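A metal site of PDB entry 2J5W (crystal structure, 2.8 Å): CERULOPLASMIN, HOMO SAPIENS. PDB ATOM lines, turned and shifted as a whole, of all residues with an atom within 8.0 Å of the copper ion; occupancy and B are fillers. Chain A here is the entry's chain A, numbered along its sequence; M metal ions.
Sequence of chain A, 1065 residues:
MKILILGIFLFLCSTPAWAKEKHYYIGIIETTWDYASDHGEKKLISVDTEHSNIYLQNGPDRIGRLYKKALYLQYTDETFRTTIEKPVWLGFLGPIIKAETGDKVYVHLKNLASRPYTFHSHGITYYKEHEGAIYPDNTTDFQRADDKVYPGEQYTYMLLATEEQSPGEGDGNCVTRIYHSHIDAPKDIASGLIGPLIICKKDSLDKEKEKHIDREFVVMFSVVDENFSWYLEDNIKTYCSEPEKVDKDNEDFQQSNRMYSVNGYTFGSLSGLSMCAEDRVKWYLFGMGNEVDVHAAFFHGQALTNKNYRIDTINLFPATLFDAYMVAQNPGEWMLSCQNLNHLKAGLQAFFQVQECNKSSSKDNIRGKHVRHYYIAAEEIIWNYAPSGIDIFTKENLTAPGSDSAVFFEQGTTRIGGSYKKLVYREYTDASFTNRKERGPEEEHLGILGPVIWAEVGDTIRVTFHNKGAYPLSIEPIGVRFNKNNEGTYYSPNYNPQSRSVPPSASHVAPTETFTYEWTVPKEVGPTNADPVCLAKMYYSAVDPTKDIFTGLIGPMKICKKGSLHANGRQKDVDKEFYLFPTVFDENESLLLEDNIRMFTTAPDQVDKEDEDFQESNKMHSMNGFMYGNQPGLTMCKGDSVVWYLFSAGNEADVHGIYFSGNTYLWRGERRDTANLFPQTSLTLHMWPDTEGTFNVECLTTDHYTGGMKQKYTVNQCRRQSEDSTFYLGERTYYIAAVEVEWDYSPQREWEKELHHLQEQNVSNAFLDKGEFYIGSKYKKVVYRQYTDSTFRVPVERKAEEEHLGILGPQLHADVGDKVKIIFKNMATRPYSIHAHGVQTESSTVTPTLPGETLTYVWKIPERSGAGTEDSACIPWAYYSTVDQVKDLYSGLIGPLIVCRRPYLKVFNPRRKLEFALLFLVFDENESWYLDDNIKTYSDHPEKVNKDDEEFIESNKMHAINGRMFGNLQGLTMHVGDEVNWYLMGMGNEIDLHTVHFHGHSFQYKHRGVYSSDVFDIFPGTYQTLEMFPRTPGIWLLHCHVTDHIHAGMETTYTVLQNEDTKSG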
ATOM      1  N   PHE A 221      -4.721 -22.896 -13.586  1.00  0.00           N
ATOM      2  CA  PHE A 221      -3.978 -22.046 -12.660  1.00  0.00           C
ATOM      3  C   PHE A 221      -4.977 -21.399 -11.712  1.00  0.00           C
ATOM      4  O   PHE A 221      -5.941 -20.775 -12.153  1.00  0.00           O
ATOM      5  CB  PHE A 221      -3.180 -20.965 -13.403  1.00  0.00           C
ATOM      6  CG  PHE A 221      -1.880 -21.454 -13.958  1.00  0.00           C
ATOM      7  CD1 PHE A 221      -1.860 -22.393 -14.991  1.00  0.00           C
ATOM      8  CD2 PHE A 221      -0.671 -20.989 -13.449  1.00  0.00           C
ATOM      9  CE1 PHE A 221      -0.662 -22.850 -15.492  1.00  0.00           C
ATOM     10  CE2 PHE A 221       0.527 -21.447 -13.951  1.00  0.00           C
ATOM     11  CZ  PHE A 221       0.526 -22.381 -14.972  1.00  0.00           C
ATOM     12  N   SER A 222      -4.770 -21.559 -10.406  1.00  0.00           N
ATOM     13  CA  SER A 222      -5.667 -20.964  -9.425  1.00  0.00           C
ATOM     14  C   SER A 222      -5.045 -20.896  -8.056  1.00  0.00           C
ATOM     15  O   SER A 222      -4.356 -21.818  -7.630  1.00  0.00           O
ATOM     16  CB  SER A 222      -6.978 -21.765  -9.301  1.00  0.00           C
ATOM     17  OG  SER A 222      -7.801 -21.231  -8.265  1.00  0.00           O
ATOM     18  N   VAL A 223      -5.303 -19.783  -7.385  1.00  0.00           N
ATOM     19  CA  VAL A 223      -5.060 -19.691  -5.971  1.00  0.00           C
ATOM     20  C   VAL A 223      -6.316 -20.297  -5.337  1.00  0.00           C
ATOM     21  O   VAL A 223      -7.259 -19.560  -5.013  1.00  0.00           O
ATOM     22  CB  VAL A 223      -4.854 -18.237  -5.529  1.00  0.00           C
ATOM     23  CG1 VAL A 223      -4.433 -18.184  -4.053  1.00  0.00           C
ATOM     24  CG2 VAL A 223      -3.824 -17.586  -6.383  1.00  0.00           C
ATOM     25  N   TYR A 260      -1.788 -21.902  -3.809  1.00  0.00           N
ATOM     26  CA  TYR A 260      -1.313 -21.509  -5.129  1.00  0.00           C
ATOM     27  C   TYR A 260      -0.877 -22.788  -5.866  1.00  0.00           C
ATOM     28  O   TYR A 260       0.164 -23.377  -5.567  1.00  0.00           O
ATOM     29  CB  TYR A 260      -0.160 -20.507  -5.029  1.00  0.00           C
ATOM     30  CG  TYR A 260      -0.485 -19.226  -4.290  1.00  0.00           C
ATOM     31  CD1 TYR A 260      -0.585 -19.209  -2.913  1.00  0.00           C
ATOM     32  CD2 TYR A 260      -0.632 -18.025  -4.966  1.00  0.00           C
ATOM     33  CE1 TYR A 260      -0.847 -18.041  -2.222  1.00  0.00           C
ATOM     34  CE2 TYR A 260      -0.899 -16.836  -4.284  1.00  0.00           C
ATOM     35  CZ  TYR A 260      -1.003 -16.862  -2.899  1.00  0.00           C
ATOM     36  OH  TYR A 260      -1.272 -15.725  -2.180  1.00  0.00           O
ATOM     37  N   SER A 261      -1.690 -23.208  -6.836  1.00  0.00           N
ATOM     38  CA  SER A 261      -1.530 -24.511  -7.416  1.00  0.00           C
ATOM     39  C   SER A 261      -1.854 -24.543  -8.890  1.00  0.00           C
ATOM     40  O   SER A 261      -2.546 -23.672  -9.412  1.00  0.00           O
ATOM     41  CB  SER A 261      -2.443 -25.474  -6.672  1.00  0.00           C
ATOM     42  OG  SER A 261      -3.774 -25.013  -6.652  1.00  0.00           O
ATOM     43  N   VAL A 292      -6.966 -11.850  -7.031  1.00  0.00           N
ATOM     44  CA  VAL A 292      -5.552 -12.289  -6.963  1.00  0.00           C
ATOM     45  C   VAL A 292      -5.156 -13.205  -8.124  1.00  0.00           C
ATOM     46  O   VAL A 292      -3.957 -13.461  -8.312  1.00  0.00           O
ATOM     47  CB  VAL A 292      -5.187 -13.055  -5.640  1.00  0.00           C
ATOM     48  CG1 VAL A 292      -5.006 -12.092  -4.493  1.00  0.00           C
ATOM     49  CG2 VAL A 292      -6.215 -14.158  -5.328  1.00  0.00           C
ATOM     50  N   ASP A 293      -6.128 -13.722  -8.870  1.00  0.00           N
ATOM     51  CA  ASP A 293      -5.806 -14.701  -9.909  1.00  0.00           C
ATOM     52  C   ASP A 293      -5.415 -14.009 -11.228  1.00  0.00           C
ATOM     53  O   ASP A 293      -6.030 -14.224 -12.277  1.00  0.00           O
ATOM     54  CB  ASP A 293      -6.909 -15.747 -10.040  1.00  0.00           C
ATOM     55  CG  ASP A 293      -6.991 -16.658  -8.811  1.00  0.00           C
ATOM     56  OD1 ASP A 293      -7.614 -16.263  -7.787  1.00  0.00           O
ATOM     57  OD2 ASP A 293      -6.435 -17.776  -8.855  1.00  0.00           O
ATOM     58  N   VAL A 294      -4.381 -13.172 -11.128  1.00  0.00           N
ATOM     59  CA  VAL A 294      -3.668 -12.650 -12.269  1.00  0.00           C
ATOM     60  C   VAL A 294      -2.519 -13.613 -12.576  1.00  0.00           C
ATOM     61  O   VAL A 294      -1.436 -13.482 -12.014  1.00  0.00           O
ATOM     62  CB  VAL A 294      -3.103 -11.259 -11.961  1.00  0.00           C
ATOM     63  CG1 VAL A 294      -2.240 -10.766 -13.120  1.00  0.00           C
ATOM     64  CG2 VAL A 294      -4.224 -10.286 -11.659  1.00  0.00           C
ATOM     65  N   HIS A 295      -2.750 -14.575 -13.451  1.00  0.00           N
ATOM     66  CA  HIS A 295      -1.736 -15.594 -13.722  1.00  0.00           C
ATOM     67  C   HIS A 295      -0.901 -15.353 -14.983  1.00  0.00           C
ATOM     68  O   HIS A 295      -1.352 -14.700 -15.944  1.00  0.00           O
ATOM     69  CB  HIS A 295      -2.401 -16.958 -13.775  1.00  0.00           C
ATOM     70  CG  HIS A 295      -3.070 -17.343 -12.498  1.00  0.00           C
ATOM     71  ND1 HIS A 295      -2.364 -17.715 -11.373  1.00  0.00           N
ATOM     72  CD2 HIS A 295      -4.381 -17.396 -12.155  1.00  0.00           C
ATOM     73  CE1 HIS A 295      -3.214 -17.975 -10.397  1.00  0.00           C
ATOM     74  NE2 HIS A 295      -4.439 -17.784 -10.848  1.00  0.00           N
ATOM     75  N   ALA A 296       0.325 -15.888 -14.974  1.00  0.00           N
ATOM     76  CA  ALA A 296       1.235 -15.743 -16.096  1.00  0.00           C
ATOM     77  C   ALA A 296       1.914 -17.067 -16.452  1.00  0.00           C
ATOM     78  O   ALA A 296       3.093 -17.267 -16.174  1.00  0.00           O
ATOM     79  CB  ALA A 296       2.267 -14.655 -15.784  1.00  0.00           C
ATOM     80  N   ALA A 297       1.159 -17.972 -17.068  1.00  0.00           N
ATOM     81  CA  ALA A 297       1.642 -19.335 -17.290  1.00  0.00           C
ATOM     82  C   ALA A 297       2.806 -19.367 -18.292  1.00  0.00           C
ATOM     83  O   ALA A 297       2.697 -18.863 -19.409  1.00  0.00           O
ATOM     84  CB  ALA A 297       0.492 -20.238 -17.754  1.00  0.00           C
ATOM     85  N   LEU A 316      -3.751 -15.793 -17.641  1.00  0.00           N
ATOM     86  CA  LEU A 316      -5.038 -16.419 -17.321  1.00  0.00           C
ATOM     87  C   LEU A 316      -5.630 -15.735 -16.117  1.00  0.00           C
ATOM     88  O   LEU A 316      -4.915 -15.356 -15.179  1.00  0.00           O
ATOM     89  CB  LEU A 316      -4.827 -17.899 -17.008  1.00  0.00           C
ATOM     90  CG  LEU A 316      -4.245 -18.738 -18.139  1.00  0.00           C
ATOM     91  CD1 LEU A 316      -3.814 -20.092 -17.609  1.00  0.00           C
ATOM     92  CD2 LEU A 316      -5.242 -18.864 -19.279  1.00  0.00           C
ATOM     93  N   SER A 337       5.682 -22.466 -14.759  1.00  0.00           N
ATOM     94  CA  SER A 337       5.482 -21.545 -13.647  1.00  0.00           C
ATOM     95  C   SER A 337       4.506 -20.425 -13.960  1.00  0.00           C
ATOM     96  O   SER A 337       4.209 -20.132 -15.114  1.00  0.00           O
ATOM     97  CB  SER A 337       6.825 -20.945 -13.211  1.00  0.00           C
ATOM     98  OG  SER A 337       7.505 -20.379 -14.309  1.00  0.00           O
ATOM     99  N   CYS A 338       3.980 -19.826 -12.894  1.00  0.00           N
ATOM    100  CA  CYS A 338       3.225 -18.595 -12.990  1.00  0.00           C
ATOM    101  C   CYS A 338       4.233 -17.509 -12.695  1.00  0.00           C
ATOM    102  O   CYS A 338       4.892 -17.546 -11.644  1.00  0.00           O
ATOM    103  CB  CYS A 338       2.097 -18.553 -11.969  1.00  0.00           C
ATOM    104  SG  CYS A 338       1.140 -17.007 -12.008  1.00  0.00           S
ATOM    105  N   GLN A 339       4.338 -16.543 -13.620  1.00  0.00           N
ATOM    106  CA  GLN A 339       5.360 -15.500 -13.548  1.00  0.00           C
ATOM    107  C   GLN A 339       4.854 -14.254 -12.830  1.00  0.00           C
ATOM    108  O   GLN A 339       5.529 -13.215 -12.773  1.00  0.00           O
ATOM    109  CB  GLN A 339       5.899 -15.218 -14.948  1.00  0.00           C
ATOM    110  CG  GLN A 339       6.673 -16.400 -15.543  1.00  0.00           C
ATOM    111  CD  GLN A 339       7.975 -16.689 -14.784  1.00  0.00           C
ATOM    112  OE1 GLN A 339       8.776 -15.786 -14.555  1.00  0.00           O
ATOM    113  NE2 GLN A 339       8.179 -17.955 -14.372  1.00  0.00           N
ATOM    114  N   ASN A 340       3.654 -14.361 -12.264  1.00  0.00           N
ATOM    115  CA  ASN A 340       3.198 -13.434 -11.259  1.00  0.00           C
ATOM    116  C   ASN A 340       4.100 -13.624 -10.059  1.00  0.00           C
ATOM    117  O   ASN A 340       4.053 -14.654  -9.415  1.00  0.00           O
ATOM    118  CB  ASN A 340       1.742 -13.743 -10.876  1.00  0.00           C
ATOM    119  CG  ASN A 340       1.205 -12.841  -9.792  1.00  0.00           C
ATOM    120  OD1 ASN A 340       1.948 -12.349  -8.934  1.00  0.00           O
ATOM    121  ND2 ASN A 340      -0.090 -12.630  -9.809  1.00  0.00           N
ATOM    122  N   LEU A 341       4.928 -12.638  -9.766  1.00  0.00           N
ATOM    123  CA  LEU A 341       6.006 -12.829  -8.806  1.00  0.00           C
ATOM    124  C   LEU A 341       5.521 -13.276  -7.421  1.00  0.00           C
ATOM    125  O   LEU A 341       6.190 -14.085  -6.768  1.00  0.00           O
ATOM    126  CB  LEU A 341       6.905 -11.583  -8.711  1.00  0.00           C
ATOM    127  CG  LEU A 341       7.618 -11.137 -10.002  1.00  0.00           C
ATOM    128  CD1 LEU A 341       8.586 -10.020  -9.689  1.00  0.00           C
ATOM    129  CD2 LEU A 341       8.342 -12.288 -10.718  1.00  0.00           C
ATOM    130  N   ASN A 342       4.355 -12.797  -6.999  1.00  0.00           N
ATOM    131  CA  ASN A 342       3.742 -13.310  -5.757  1.00  0.00           C
ATOM    132  C   ASN A 342       3.361 -14.784  -5.855  1.00  0.00           C
ATOM    133  O   ASN A 342       3.559 -15.556  -4.898  1.00  0.00           O
ATOM    134  CB  ASN A 342       2.540 -12.477  -5.355  1.00  0.00           C
ATOM    135  CG  ASN A 342       2.922 -11.138  -4.774  1.00  0.00           C
ATOM    136  OD1 ASN A 342       4.060 -10.952  -4.341  1.00  0.00           O
ATOM    137  ND2 ASN A 342       1.988 -10.204  -4.762  1.00  0.00           N
ATOM    138  N   HIS A 343       2.832 -15.192  -6.995  1.00  0.00           N
ATOM    139  CA  HIS A 343       2.457 -16.582  -7.192  1.00  0.00           C
ATOM    140  C   HIS A 343       3.701 -17.487  -7.274  1.00  0.00           C
ATOM    141  O   HIS A 343       3.701 -18.611  -6.774  1.00  0.00           O
ATOM    142  CB  HIS A 343       1.584 -16.755  -8.448  1.00  0.00           C
ATOM    143  CG  HIS A 343       0.269 -16.033  -8.378  1.00  0.00           C
ATOM    144  ND1 HIS A 343      -0.716 -16.206  -9.312  1.00  0.00           N
ATOM    145  CD2 HIS A 343      -0.217 -15.130  -7.484  1.00  0.00           C
ATOM    146  CE1 HIS A 343      -1.754 -15.454  -9.011  1.00  0.00           C
ATOM    147  NE2 HIS A 343      -1.474 -14.793  -7.899  1.00  0.00           N
ATOM    148  N   LEU A 344       4.759 -16.969  -7.886  1.00  0.00           N
ATOM    149  CA  LEU A 344       6.009 -17.725  -8.069  1.00  0.00           C
ATOM    150  C   LEU A 344       6.578 -18.031  -6.694  1.00  0.00           C
ATOM    151  O   LEU A 344       6.902 -19.189  -6.366  1.00  0.00           O
ATOM    152  CB  LEU A 344       7.018 -16.919  -8.919  1.00  0.00           C
ATOM    153  CG  LEU A 344       8.272 -17.656  -9.431  1.00  0.00           C
ATOM    154  CD1 LEU A 344       7.920 -18.716 -10.493  1.00  0.00           C
ATOM    155  CD2 LEU A 344       9.318 -16.653  -9.968  1.00  0.00           C
ATOM    156  N   LEU A 348       3.792 -21.388  -7.032  1.00  0.00           N
ATOM    157  CA  LEU A 348       2.920 -21.862  -8.121  1.00  0.00           C
ATOM    158  C   LEU A 348       3.767 -22.357  -9.311  1.00  0.00           C
ATOM    159  O   LEU A 348       3.952 -21.665 -10.315  1.00  0.00           O
ATOM    160  CB  LEU A 348       1.908 -20.796  -8.536  1.00  0.00           C
ATOM    161  CG  LEU A 348       0.606 -21.354  -9.149  1.00  0.00           C
ATOM    162  CD1 LEU A 348      -0.401 -20.236  -9.353  1.00  0.00           C
ATOM    163  CD2 LEU A 348       0.867 -22.087 -10.457  1.00  0.00           C
ATOM    164  N   GLU A 652       0.013  -9.277  -9.186  1.00  0.00           N
ATOM    165  CA  GLU A 652      -1.396  -8.970  -9.424  1.00  0.00           C
ATOM    166  C   GLU A 652      -1.733  -7.469  -9.546  1.00  0.00           C
ATOM    167  O   GLU A 652      -2.760  -7.118 -10.143  1.00  0.00           O
ATOM    168  CB  GLU A 652      -2.280  -9.636  -8.362  1.00  0.00           C
ATOM    169  CG  GLU A 652      -1.862  -9.390  -6.909  1.00  0.00           C
ATOM    170  CD  GLU A 652      -0.969 -10.483  -6.329  1.00  0.00           C
ATOM    171  OE1 GLU A 652      -0.568 -11.439  -7.036  1.00  0.00           O
ATOM    172  OE2 GLU A 652      -0.672 -10.366  -5.128  1.00  0.00           O
ATOM    173  N   PRO A 679       1.761  -9.527 -15.841  1.00  0.00           N
ATOM    174  CA  PRO A 679       3.128 -10.019 -15.637  1.00  0.00           C
ATOM    175  C   PRO A 679       3.643 -10.831 -16.831  1.00  0.00           C
ATOM    176  O   PRO A 679       2.930 -11.719 -17.319  1.00  0.00           O
ATOM    177  CB  PRO A 679       3.014 -10.884 -14.382  1.00  0.00           C
ATOM    178  CG  PRO A 679       1.870 -10.287 -13.641  1.00  0.00           C
ATOM    179  CD  PRO A 679       0.873  -9.953 -14.753  1.00  0.00           C
HETATM  180 CU    CU M   1      -0.485 -17.106 -10.960  1.00  0.00          CU
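The copper ion is bound by ND1 of His 343 (1.9 Å), SG of Cys 338 (1.9 Å) and ND1 of His 295 (2.0 Å). The copper ion has three donor atoms within binding distance.
ND2 of Asn 340 is in hydrogen-bond range of O of Val 294 (2.7 Å). The side-chain sulfur (SG) of Cys 338 lies close to the backbone NH (N) of Ala 296 (3.3 Å). NE2 of His 295 lies within hydrogen-bond range of OD2 of Asp 293 (2.8 Å). A ring nitrogen (NE2) of His 343 is in hydrogen-bond range of the side-chain amide nitrogen (ND2) of Asn 340, at 3.2 Å. A ring nitrogen (NE2) of His 343 lies within hydrogen-bond range of the backbone carbonyl oxygen (O) of Val 292 (2.8 Å). The side-chain sulfur (SG) of Cys 338 lies close to the backbone NH (N) of Asn 340, at 3.7 Å. The backbone NH (N) of His 295 lies within hydrogen-bond range of the backbone carbonyl oxygen (O) of Leu 316, 2.9 Å away. The backbone carbonyl oxygen of His 343 sits at hydrogen-bond distance from the backbone NH of Leu 348.
Val 294 touches the copper ion. Leu 348 touches the copper ion (CD1 to CU, 3.5 Å). Five residues have an atom within 4 Å of the copper ion: Val 294, His 295, Cys 338, His 343 and Leu 348.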
